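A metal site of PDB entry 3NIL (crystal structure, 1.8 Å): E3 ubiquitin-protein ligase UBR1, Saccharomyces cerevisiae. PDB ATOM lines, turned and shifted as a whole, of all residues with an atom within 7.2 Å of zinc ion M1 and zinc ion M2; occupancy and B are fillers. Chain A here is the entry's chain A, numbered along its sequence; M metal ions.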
ATOM      1  N   HIS A   4     -17.989  31.557  32.259  1.00  0.00           N
ATOM      2  CA  HIS A   4     -16.571  31.891  32.243  1.00  0.00           C
ATOM      3  C   HIS A   4     -16.034  31.771  30.822  1.00  0.00           C
ATOM      4  O   HIS A   4     -16.299  30.786  30.141  1.00  0.00           O
ATOM      5  CB  HIS A   4     -15.807  30.973  33.202  1.00  0.00           C
ATOM      6  CG  HIS A   4     -14.386  31.380  33.416  1.00  0.00           C
ATOM      7  ND1 HIS A   4     -13.439  30.521  33.923  1.00  0.00           N
ATOM      8  CD2 HIS A   4     -13.742  32.562  33.211  1.00  0.00           C
ATOM      9  CE1 HIS A   4     -12.272  31.147  34.024  1.00  0.00           C
ATOM     10  NE2 HIS A   4     -12.437  32.384  33.601  1.00  0.00           N
ATOM     11  N   LYS A   5     -15.325  32.809  30.370  1.00  0.00           N
ATOM     12  CA  LYS A   5     -14.695  32.798  29.058  1.00  0.00           C
ATOM     13  C   LYS A   5     -13.406  31.974  29.132  1.00  0.00           C
ATOM     14  O   LYS A   5     -12.779  31.881  30.176  1.00  0.00           O
ATOM     15  CB  LYS A   5     -14.360  34.219  28.608  1.00  0.00           C
ATOM     16  CG  LYS A   5     -15.575  35.149  28.482  1.00  0.00           C
ATOM     17  CD  LYS A   5     -15.134  36.514  27.990  1.00  0.00           C
ATOM     18  CE  LYS A   5     -16.271  37.520  27.995  1.00  0.00           C
ATOM     19  NZ  LYS A   5     -15.782  38.830  27.439  1.00  0.00           N
ATOM     20  N   HIS A   6     -13.041  31.351  28.015  1.00  0.00           N
ATOM     21  CA  HIS A   6     -11.806  30.583  27.942  1.00  0.00           C
ATOM     22  C   HIS A   6     -10.893  31.139  26.852  1.00  0.00           C
ATOM     23  O   HIS A   6     -10.275  30.395  26.094  1.00  0.00           O
ATOM     24  CB  HIS A   6     -12.107  29.092  27.718  1.00  0.00           C
ATOM     25  CG  HIS A   6     -12.827  28.794  26.434  1.00  0.00           C
ATOM     26  ND1 HIS A   6     -12.160  28.543  25.258  1.00  0.00           N
ATOM     27  CD2 HIS A   6     -14.142  28.667  26.166  1.00  0.00           C
ATOM     28  CE1 HIS A   6     -13.044  28.281  24.300  1.00  0.00           C
ATOM     29  NE2 HIS A   6     -14.256  28.362  24.825  1.00  0.00           N
ATOM     30  N   ARG A   9      -7.532  29.797  24.696  1.00  0.00           N
ATOM     31  CA  ARG A   9      -7.356  28.357  24.917  1.00  0.00           C
ATOM     32  C   ARG A   9      -8.631  27.608  24.581  1.00  0.00           C
ATOM     33  O   ARG A   9      -9.627  28.204  24.194  1.00  0.00           O
ATOM     34  CB  ARG A   9      -6.929  28.046  26.365  1.00  0.00           C
ATOM     35  CG  ARG A   9      -7.897  28.538  27.434  1.00  0.00           C
ATOM     36  CD  ARG A   9      -7.722  27.797  28.743  1.00  0.00           C
ATOM     37  NE  ARG A   9      -8.501  26.552  28.778  1.00  0.00           N
ATOM     38  CZ  ARG A   9      -8.610  25.758  29.835  1.00  0.00           C
ATOM     39  NH1 ARG A   9      -7.977  26.037  30.976  1.00  0.00           N
ATOM     40  NH2 ARG A   9      -9.354  24.671  29.752  1.00  0.00           N
ATOM     41  N   ASN A  10      -8.596  26.299  24.713  1.00  0.00           N
ATOM     42  CA  ASN A  10      -9.762  25.482  24.458  1.00  0.00           C
ATOM     43  C   ASN A  10     -10.685  25.532  25.665  1.00  0.00           C
ATOM     44  O   ASN A  10     -10.281  25.916  26.771  1.00  0.00           O
ATOM     45  CB  ASN A  10      -9.329  24.037  24.202  1.00  0.00           C
ATOM     46  CG  ASN A  10      -8.797  23.391  25.434  1.00  0.00           C
ATOM     47  OD1 ASN A  10      -7.855  23.890  26.049  1.00  0.00           O
ATOM     48  ND2 ASN A  10      -9.399  22.289  25.839  1.00  0.00           N
ATOM     49  N   CYS A  11     -11.937  25.148  25.460  1.00  0.00           N
ATOM     50  CA  CYS A  11     -12.883  25.064  26.549  1.00  0.00           C
ATOM     51  C   CYS A  11     -12.546  23.842  27.431  1.00  0.00           C
ATOM     52  O   CYS A  11     -12.193  23.975  28.622  1.00  0.00           O
ATOM     53  CB  CYS A  11     -14.309  25.019  25.990  1.00  0.00           C
ATOM     54  SG  CYS A  11     -15.522  24.645  27.246  1.00  0.00           S
ATOM     55  N   GLY A  12     -12.671  22.655  26.849  1.00  0.00           N
ATOM     56  CA  GLY A  12     -12.358  21.416  27.555  1.00  0.00           C
ATOM     57  C   GLY A  12     -13.281  21.039  28.708  1.00  0.00           C
ATOM     58  O   GLY A  12     -12.979  20.114  29.463  1.00  0.00           O
ATOM     59  N   ARG A  13     -14.406  21.731  28.855  1.00  0.00           N
ATOM     60  CA  ARG A  13     -15.356  21.453  29.932  1.00  0.00           C
ATOM     61  C   ARG A  13     -15.874  20.033  29.813  1.00  0.00           C
ATOM     62  O   ARG A  13     -16.337  19.625  28.753  1.00  0.00           O
ATOM     63  CB  ARG A  13     -16.534  22.436  29.833  1.00  0.00           C
ATOM     64  CG  ARG A  13     -17.452  22.471  31.029  1.00  0.00           C
ATOM     65  CD  ARG A  13     -18.453  23.608  30.866  1.00  0.00           C
ATOM     66  NE  ARG A  13     -19.586  23.498  31.787  1.00  0.00           N
ATOM     67  CZ  ARG A  13     -20.597  22.643  31.639  1.00  0.00           C
ATOM     68  NH1 ARG A  13     -21.585  22.636  32.520  1.00  0.00           N
ATOM     69  NH2 ARG A  13     -20.628  21.809  30.604  1.00  0.00           N
ATOM     70  N   PHE A  15     -18.673  17.496  30.262  1.00  0.00           N
ATOM     71  CA  PHE A  15     -20.134  17.525  30.336  1.00  0.00           C
ATOM     72  C   PHE A  15     -20.624  16.904  31.647  1.00  0.00           C
ATOM     73  O   PHE A  15     -20.040  15.952  32.156  1.00  0.00           O
ATOM     74  CB  PHE A  15     -20.729  16.812  29.130  1.00  0.00           C
ATOM     75  CG  PHE A  15     -20.441  17.509  27.834  1.00  0.00           C
ATOM     76  CD1 PHE A  15     -21.260  18.539  27.381  1.00  0.00           C
ATOM     77  CD2 PHE A  15     -19.337  17.141  27.077  1.00  0.00           C
ATOM     78  CE1 PHE A  15     -20.983  19.187  26.183  1.00  0.00           C
ATOM     79  CE2 PHE A  15     -19.049  17.781  25.878  1.00  0.00           C
ATOM     80  CZ  PHE A  15     -19.868  18.810  25.425  1.00  0.00           C
ATOM     81  N   VAL A  34     -17.537  17.973  19.657  1.00  0.00           N
ATOM     82  CA  VAL A  34     -18.718  18.500  20.360  1.00  0.00           C
ATOM     83  C   VAL A  34     -18.514  19.873  21.008  1.00  0.00           C
ATOM     84  O   VAL A  34     -17.374  20.331  21.209  1.00  0.00           O
ATOM     85  CB  VAL A  34     -19.233  17.514  21.435  1.00  0.00           C
ATOM     86  CG1 VAL A  34     -19.818  16.264  20.763  1.00  0.00           C
ATOM     87  CG2 VAL A  34     -18.154  17.159  22.441  1.00  0.00           C
ATOM     88  N   LEU A  35     -19.646  20.513  21.311  1.00  0.00           N
ATOM     89  CA  LEU A  35     -19.664  21.841  21.942  1.00  0.00           C
ATOM     90  C   LEU A  35     -20.627  21.859  23.111  1.00  0.00           C
ATOM     91  O   LEU A  35     -21.725  21.289  23.044  1.00  0.00           O
ATOM     92  CB  LEU A  35     -20.119  22.907  20.923  1.00  0.00           C
ATOM     93  CG  LEU A  35     -19.097  23.164  19.813  1.00  0.00           C
ATOM     94  CD1 LEU A  35     -19.661  24.007  18.646  1.00  0.00           C
ATOM     95  CD2 LEU A  35     -17.873  23.840  20.406  1.00  0.00           C
ATOM     96  N   CYS A  36     -20.217  22.535  24.184  1.00  0.00           N
ATOM     97  CA  CYS A  36     -21.043  22.647  25.374  1.00  0.00           C
ATOM     98  C   CYS A  36     -22.009  23.824  25.239  1.00  0.00           C
ATOM     99  O   CYS A  36     -21.864  24.631  24.334  1.00  0.00           O
ATOM    100  CB  CYS A  36     -20.181  22.798  26.633  1.00  0.00           C
ATOM    101  SG  CYS A  36     -19.530  24.437  26.895  1.00  0.00           S
ATOM    102  N   ILE A  37     -22.977  23.903  26.148  1.00  0.00           N
ATOM    103  CA  ILE A  37     -24.007  24.968  26.110  1.00  0.00           C
ATOM    104  C   ILE A  37     -23.461  26.376  26.412  1.00  0.00           C
ATOM    105  O   ILE A  37     -24.062  27.378  26.055  1.00  0.00           O
ATOM    106  CB  ILE A  37     -25.251  24.607  26.990  1.00  0.00           C
ATOM    107  CG1 ILE A  37     -26.445  25.525  26.645  1.00  0.00           C
ATOM    108  CG2 ILE A  37     -24.920  24.652  28.487  1.00  0.00           C
ATOM    109  CD1 ILE A  37     -27.810  24.900  26.908  1.00  0.00           C
ATOM    110  N   HIS A  38     -22.293  26.432  27.056  1.00  0.00           N
ATOM    111  CA  HIS A  38     -21.612  27.699  27.304  1.00  0.00           C
ATOM    112  C   HIS A  38     -21.049  28.273  25.996  1.00  0.00           C
ATOM    113  O   HIS A  38     -20.961  29.503  25.827  1.00  0.00           O
ATOM    114  CB  HIS A  38     -20.449  27.502  28.295  1.00  0.00           C
ATOM    115  CG  HIS A  38     -20.862  26.993  29.634  1.00  0.00           C
ATOM    116  ND1 HIS A  38     -20.051  27.091  30.740  1.00  0.00           N
ATOM    117  CD2 HIS A  38     -22.002  26.373  30.055  1.00  0.00           C
ATOM    118  CE1 HIS A  38     -20.657  26.555  31.789  1.00  0.00           C
ATOM    119  NE2 HIS A  38     -21.842  26.110  31.395  1.00  0.00           N
ATOM    120  N   CYS A  39     -20.689  27.372  25.087  1.00  0.00           N
ATOM    121  CA  CYS A  39     -19.908  27.714  23.916  1.00  0.00           C
ATOM    122  C   CYS A  39     -20.690  27.755  22.612  1.00  0.00           C
ATOM    123  O   CYS A  39     -20.406  28.600  21.754  1.00  0.00           O
ATOM    124  CB  CYS A  39     -18.750  26.729  23.766  1.00  0.00           C
ATOM    125  SG  CYS A  39     -17.554  26.965  25.058  1.00  0.00           S
ATOM    126  N   PHE A  40     -21.612  26.819  22.448  1.00  0.00           N
ATOM    127  CA  PHE A  40     -22.353  26.671  21.194  1.00  0.00           C
ATOM    128  C   PHE A  40     -23.045  27.983  20.847  1.00  0.00           C
ATOM    129  O   PHE A  40     -23.768  28.547  21.677  1.00  0.00           O
ATOM    130  CB  PHE A  40     -23.355  25.529  21.270  1.00  0.00           C
ATOM    131  CG  PHE A  40     -24.204  25.392  20.032  1.00  0.00           C
ATOM    132  CD1 PHE A  40     -23.750  24.636  18.954  1.00  0.00           C
ATOM    133  CD2 PHE A  40     -25.472  25.997  19.954  1.00  0.00           C
ATOM    134  CE1 PHE A  40     -24.534  24.488  17.806  1.00  0.00           C
ATOM    135  CE2 PHE A  40     -26.244  25.862  18.809  1.00  0.00           C
ATOM    136  CZ  PHE A  40     -25.786  25.112  17.725  1.00  0.00           C
ATOM    137  N   ILE A  62     -15.649  16.020  26.644  1.00  0.00           N
ATOM    138  CA  ILE A  62     -15.250  17.382  26.888  1.00  0.00           C
ATOM    139  C   ILE A  62     -15.512  18.220  25.640  1.00  0.00           C
ATOM    140  O   ILE A  62     -15.520  17.706  24.504  1.00  0.00           O
ATOM    141  CB  ILE A  62     -13.755  17.497  27.287  1.00  0.00           C
ATOM    142  CG1 ILE A  62     -12.850  16.947  26.172  1.00  0.00           C
ATOM    143  CG2 ILE A  62     -13.505  16.775  28.630  1.00  0.00           C
ATOM    144  CD1 ILE A  62     -11.774  17.900  25.755  1.00  0.00           C
ATOM    145  N   CYS A  63     -15.730  19.515  25.883  1.00  0.00           N
ATOM    146  CA  CYS A  63     -16.088  20.456  24.843  1.00  0.00           C
ATOM    147  C   CYS A  63     -14.855  20.839  24.034  1.00  0.00           C
ATOM    148  O   CYS A  63     -13.789  21.084  24.590  1.00  0.00           O
ATOM    149  CB  CYS A  63     -16.733  21.705  25.486  1.00  0.00           C
ATOM    150  SG  CYS A  63     -16.967  23.064  24.347  1.00  0.00           S
ATOM    151  N   ASP A  64     -15.003  20.849  22.699  1.00  0.00           N
ATOM    152  CA  ASP A  64     -13.885  21.097  21.774  1.00  0.00           C
ATOM    153  C   ASP A  64     -13.791  22.545  21.272  1.00  0.00           C
ATOM    154  O   ASP A  64     -12.957  22.865  20.409  1.00  0.00           O
ATOM    155  CB  ASP A  64     -13.950  20.156  20.563  1.00  0.00           C
ATOM    156  CG  ASP A  64     -13.912  18.693  20.959  1.00  0.00           C
ATOM    157  OD1 ASP A  64     -12.964  18.273  21.678  1.00  0.00           O
ATOM    158  OD2 ASP A  64     -14.833  17.947  20.552  1.00  0.00           O
ATOM    159  N   CYS A  65     -14.637  23.436  21.782  1.00  0.00           N
ATOM    160  CA  CYS A  65     -14.562  24.845  21.395  1.00  0.00           C
ATOM    161  C   CYS A  65     -13.149  25.398  21.614  1.00  0.00           C
ATOM    162  O   CYS A  65     -12.569  25.221  22.687  1.00  0.00           O
ATOM    163  CB  CYS A  65     -15.585  25.650  22.206  1.00  0.00           C
ATOM    164  SG  CYS A  65     -15.676  27.398  21.780  1.00  0.00           S
ATOM    165  N   GLY A  66     -12.607  26.062  20.610  1.00  0.00           N
ATOM    166  CA  GLY A  66     -11.267  26.632  20.710  1.00  0.00           C
ATOM    167  C   GLY A  66     -10.133  25.630  20.560  1.00  0.00           C
ATOM    168  O   GLY A  66      -8.974  25.991  20.745  1.00  0.00           O
ATOM    169  N   LEU A  75     -15.244  29.173  14.842  1.00  0.00           N
ATOM    170  CA  LEU A  75     -16.359  29.340  15.769  1.00  0.00           C
ATOM    171  C   LEU A  75     -16.238  30.659  16.479  1.00  0.00           C
ATOM    172  O   LEU A  75     -15.149  31.182  16.661  1.00  0.00           O
ATOM    173  CB  LEU A  75     -16.396  28.242  16.836  1.00  0.00           C
ATOM    174  CG  LEU A  75     -16.468  26.795  16.353  1.00  0.00           C
ATOM    175  CD1 LEU A  75     -16.567  25.882  17.560  1.00  0.00           C
ATOM    176  CD2 LEU A  75     -17.672  26.610  15.440  1.00  0.00           C
ATOM    177  N   HIS A  76     -17.389  31.170  16.920  1.00  0.00           N
ATOM    178  CA  HIS A  76     -17.459  32.381  17.712  1.00  0.00           C
ATOM    179  C   HIS A  76     -18.101  32.000  19.021  1.00  0.00           C
ATOM    180  O   HIS A  76     -19.313  32.009  19.158  1.00  0.00           O
ATOM    181  CB  HIS A  76     -18.291  33.421  16.979  1.00  0.00           C
ATOM    182  CG  HIS A  76     -17.746  33.735  15.623  1.00  0.00           C
ATOM    183  ND1 HIS A  76     -18.236  33.139  14.482  1.00  0.00           N
ATOM    184  CD2 HIS A  76     -16.726  34.528  15.235  1.00  0.00           C
ATOM    185  CE1 HIS A  76     -17.555  33.578  13.438  1.00  0.00           C
ATOM    186  NE2 HIS A  76     -16.631  34.425  13.863  1.00  0.00           N
ATOM    187  N   CYS A  77     -17.257  31.614  19.971  1.00  0.00           N
ATOM    188  CA  CYS A  77     -17.722  31.107  21.237  1.00  0.00           C
ATOM    189  C   CYS A  77     -18.795  32.025  21.821  1.00  0.00           C
ATOM    190  O   CYS A  77     -18.605  33.222  21.907  1.00  0.00           O
ATOM    191  CB  CYS A  77     -16.531  31.026  22.200  1.00  0.00           C
ATOM    192  SG  CYS A  77     -16.929  30.446  23.869  1.00  0.00           S
ATOM    193  N   LYS A  78     -19.932  31.446  22.222  1.00  0.00           N
ATOM    194  CA  LYS A  78     -21.021  32.231  22.827  1.00  0.00           C
ATOM    195  C   LYS A  78     -20.588  33.010  24.078  1.00  0.00           C
ATOM    196  O   LYS A  78     -21.058  34.136  24.309  1.00  0.00           O
ATOM    197  CB  LYS A  78     -22.233  31.341  23.126  1.00  0.00           C
ATOM    198  CG  LYS A  78     -23.546  32.088  23.411  1.00  0.00           C
ATOM    199  CD  LYS A  78     -24.707  31.087  23.498  1.00  0.00           C
ATOM    200  CE  LYS A  78     -26.045  31.778  23.467  1.00  0.00           C
ATOM    201  NZ  LYS A  78     -26.236  32.636  24.651  1.00  0.00           N
ATOM    202  N   ALA A  79     -19.689  32.432  24.877  1.00  0.00           N
ATOM    203  CA  ALA A  79     -19.227  33.082  26.107  1.00  0.00           C
ATOM    204  C   ALA A  79     -18.568  34.453  25.874  1.00  0.00           C
ATOM    205  O   ALA A  79     -18.558  35.314  26.758  1.00  0.00           O
ATOM    206  CB  ALA A  79     -18.284  32.158  26.894  1.00  0.00           C
ATOM    207  N   GLU A  80     -18.028  34.651  24.676  1.00  0.00           N
ATOM    208  CA  GLU A  80     -17.359  35.913  24.353  1.00  0.00           C
ATOM    209  C   GLU A  80     -18.351  37.050  24.107  1.00  0.00           C
ATOM    210  O   GLU A  80     -17.970  38.228  24.147  1.00  0.00           O
ATOM    211  CB  GLU A  80     -16.457  35.729  23.132  1.00  0.00           C
ATOM    212  CG  GLU A  80     -15.361  34.679  23.328  1.00  0.00           C
ATOM    213  CD  GLU A  80     -14.215  35.166  24.205  1.00  0.00           C
ATOM    214  OE1 GLU A  80     -14.063  36.396  24.371  1.00  0.00           O
ATOM    215  OE2 GLU A  80     -13.466  34.310  24.726  1.00  0.00           O
HETATM  216 ZN    ZN M   1     -16.126  28.336  23.859  1.00  0.00          ZN
HETATM  217 ZN    ZN M   2     -17.417  24.677  25.948  1.00  0.00          ZN
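Of the 27 residues printed, 4 come within 4 Å of zinc ion M1. The nearest printed residue that does not touch zinc ion M1 is Cys 11 (4.3 Å).
A ring nitrogen (NE2) of His 6 is bound to zinc ion M1 (2.1 Å). SG of Cys 77 binds zinc ion M1, at 2.3 Å. SG of Cys 39 binds zinc ion M1 (2.3 Å). Zinc ion M1 is bound by the side-chain sulfur (SG) of Cys 65 (2.3 Å). Zinc ion M1 has four donor atoms within binding distance.
SG of Cys 11 binds zinc ion M2. SG of Cys 63 is bound to zinc ion M2, 2.3 Å away. The side-chain sulfur (SG) of Cys 36 is bound to zinc ion M2, 2.3 Å away. Zinc ion M2 is bound by the side-chain sulfur (SG) of Cys 39, at 2.5 Å. Zinc ion M2 has four donor atoms within binding distance.
The guanidinium group (NH2) of Arg 9 lies within hydrogen-bond range of the backbone carbonyl oxygen (O) of Cys 11 (3.1 Å). N of Gly 12 sits at hydrogen-bond distance from O of Cys 63, 3.0 Å away. A ring nitrogen (ND1) of His 6 lies within hydrogen-bond range of the backbone NH of Cys 11 (3.4 Å). N of His 38 lies close to SG of Cys 36. The backbone NH (N) of Lys 78 sits at hydrogen-bond distance from the backbone carbonyl oxygen (O) of Cys 39, 2.9 Å away. N of Cys 65 lies close to SG of Cys 63 (3.5 Å). ND1 of His 6 is in hydrogen-bond range of O of Arg 9 (2.8 Å). The backbone carbonyl oxygen of Arg 13 sits at hydrogen-bond distance from the backbone NH of Cys 63.
Four residues have an atom within 4 Å of zinc ion M2: Cys 11, Cys 36, Cys 39 and Cys 63.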
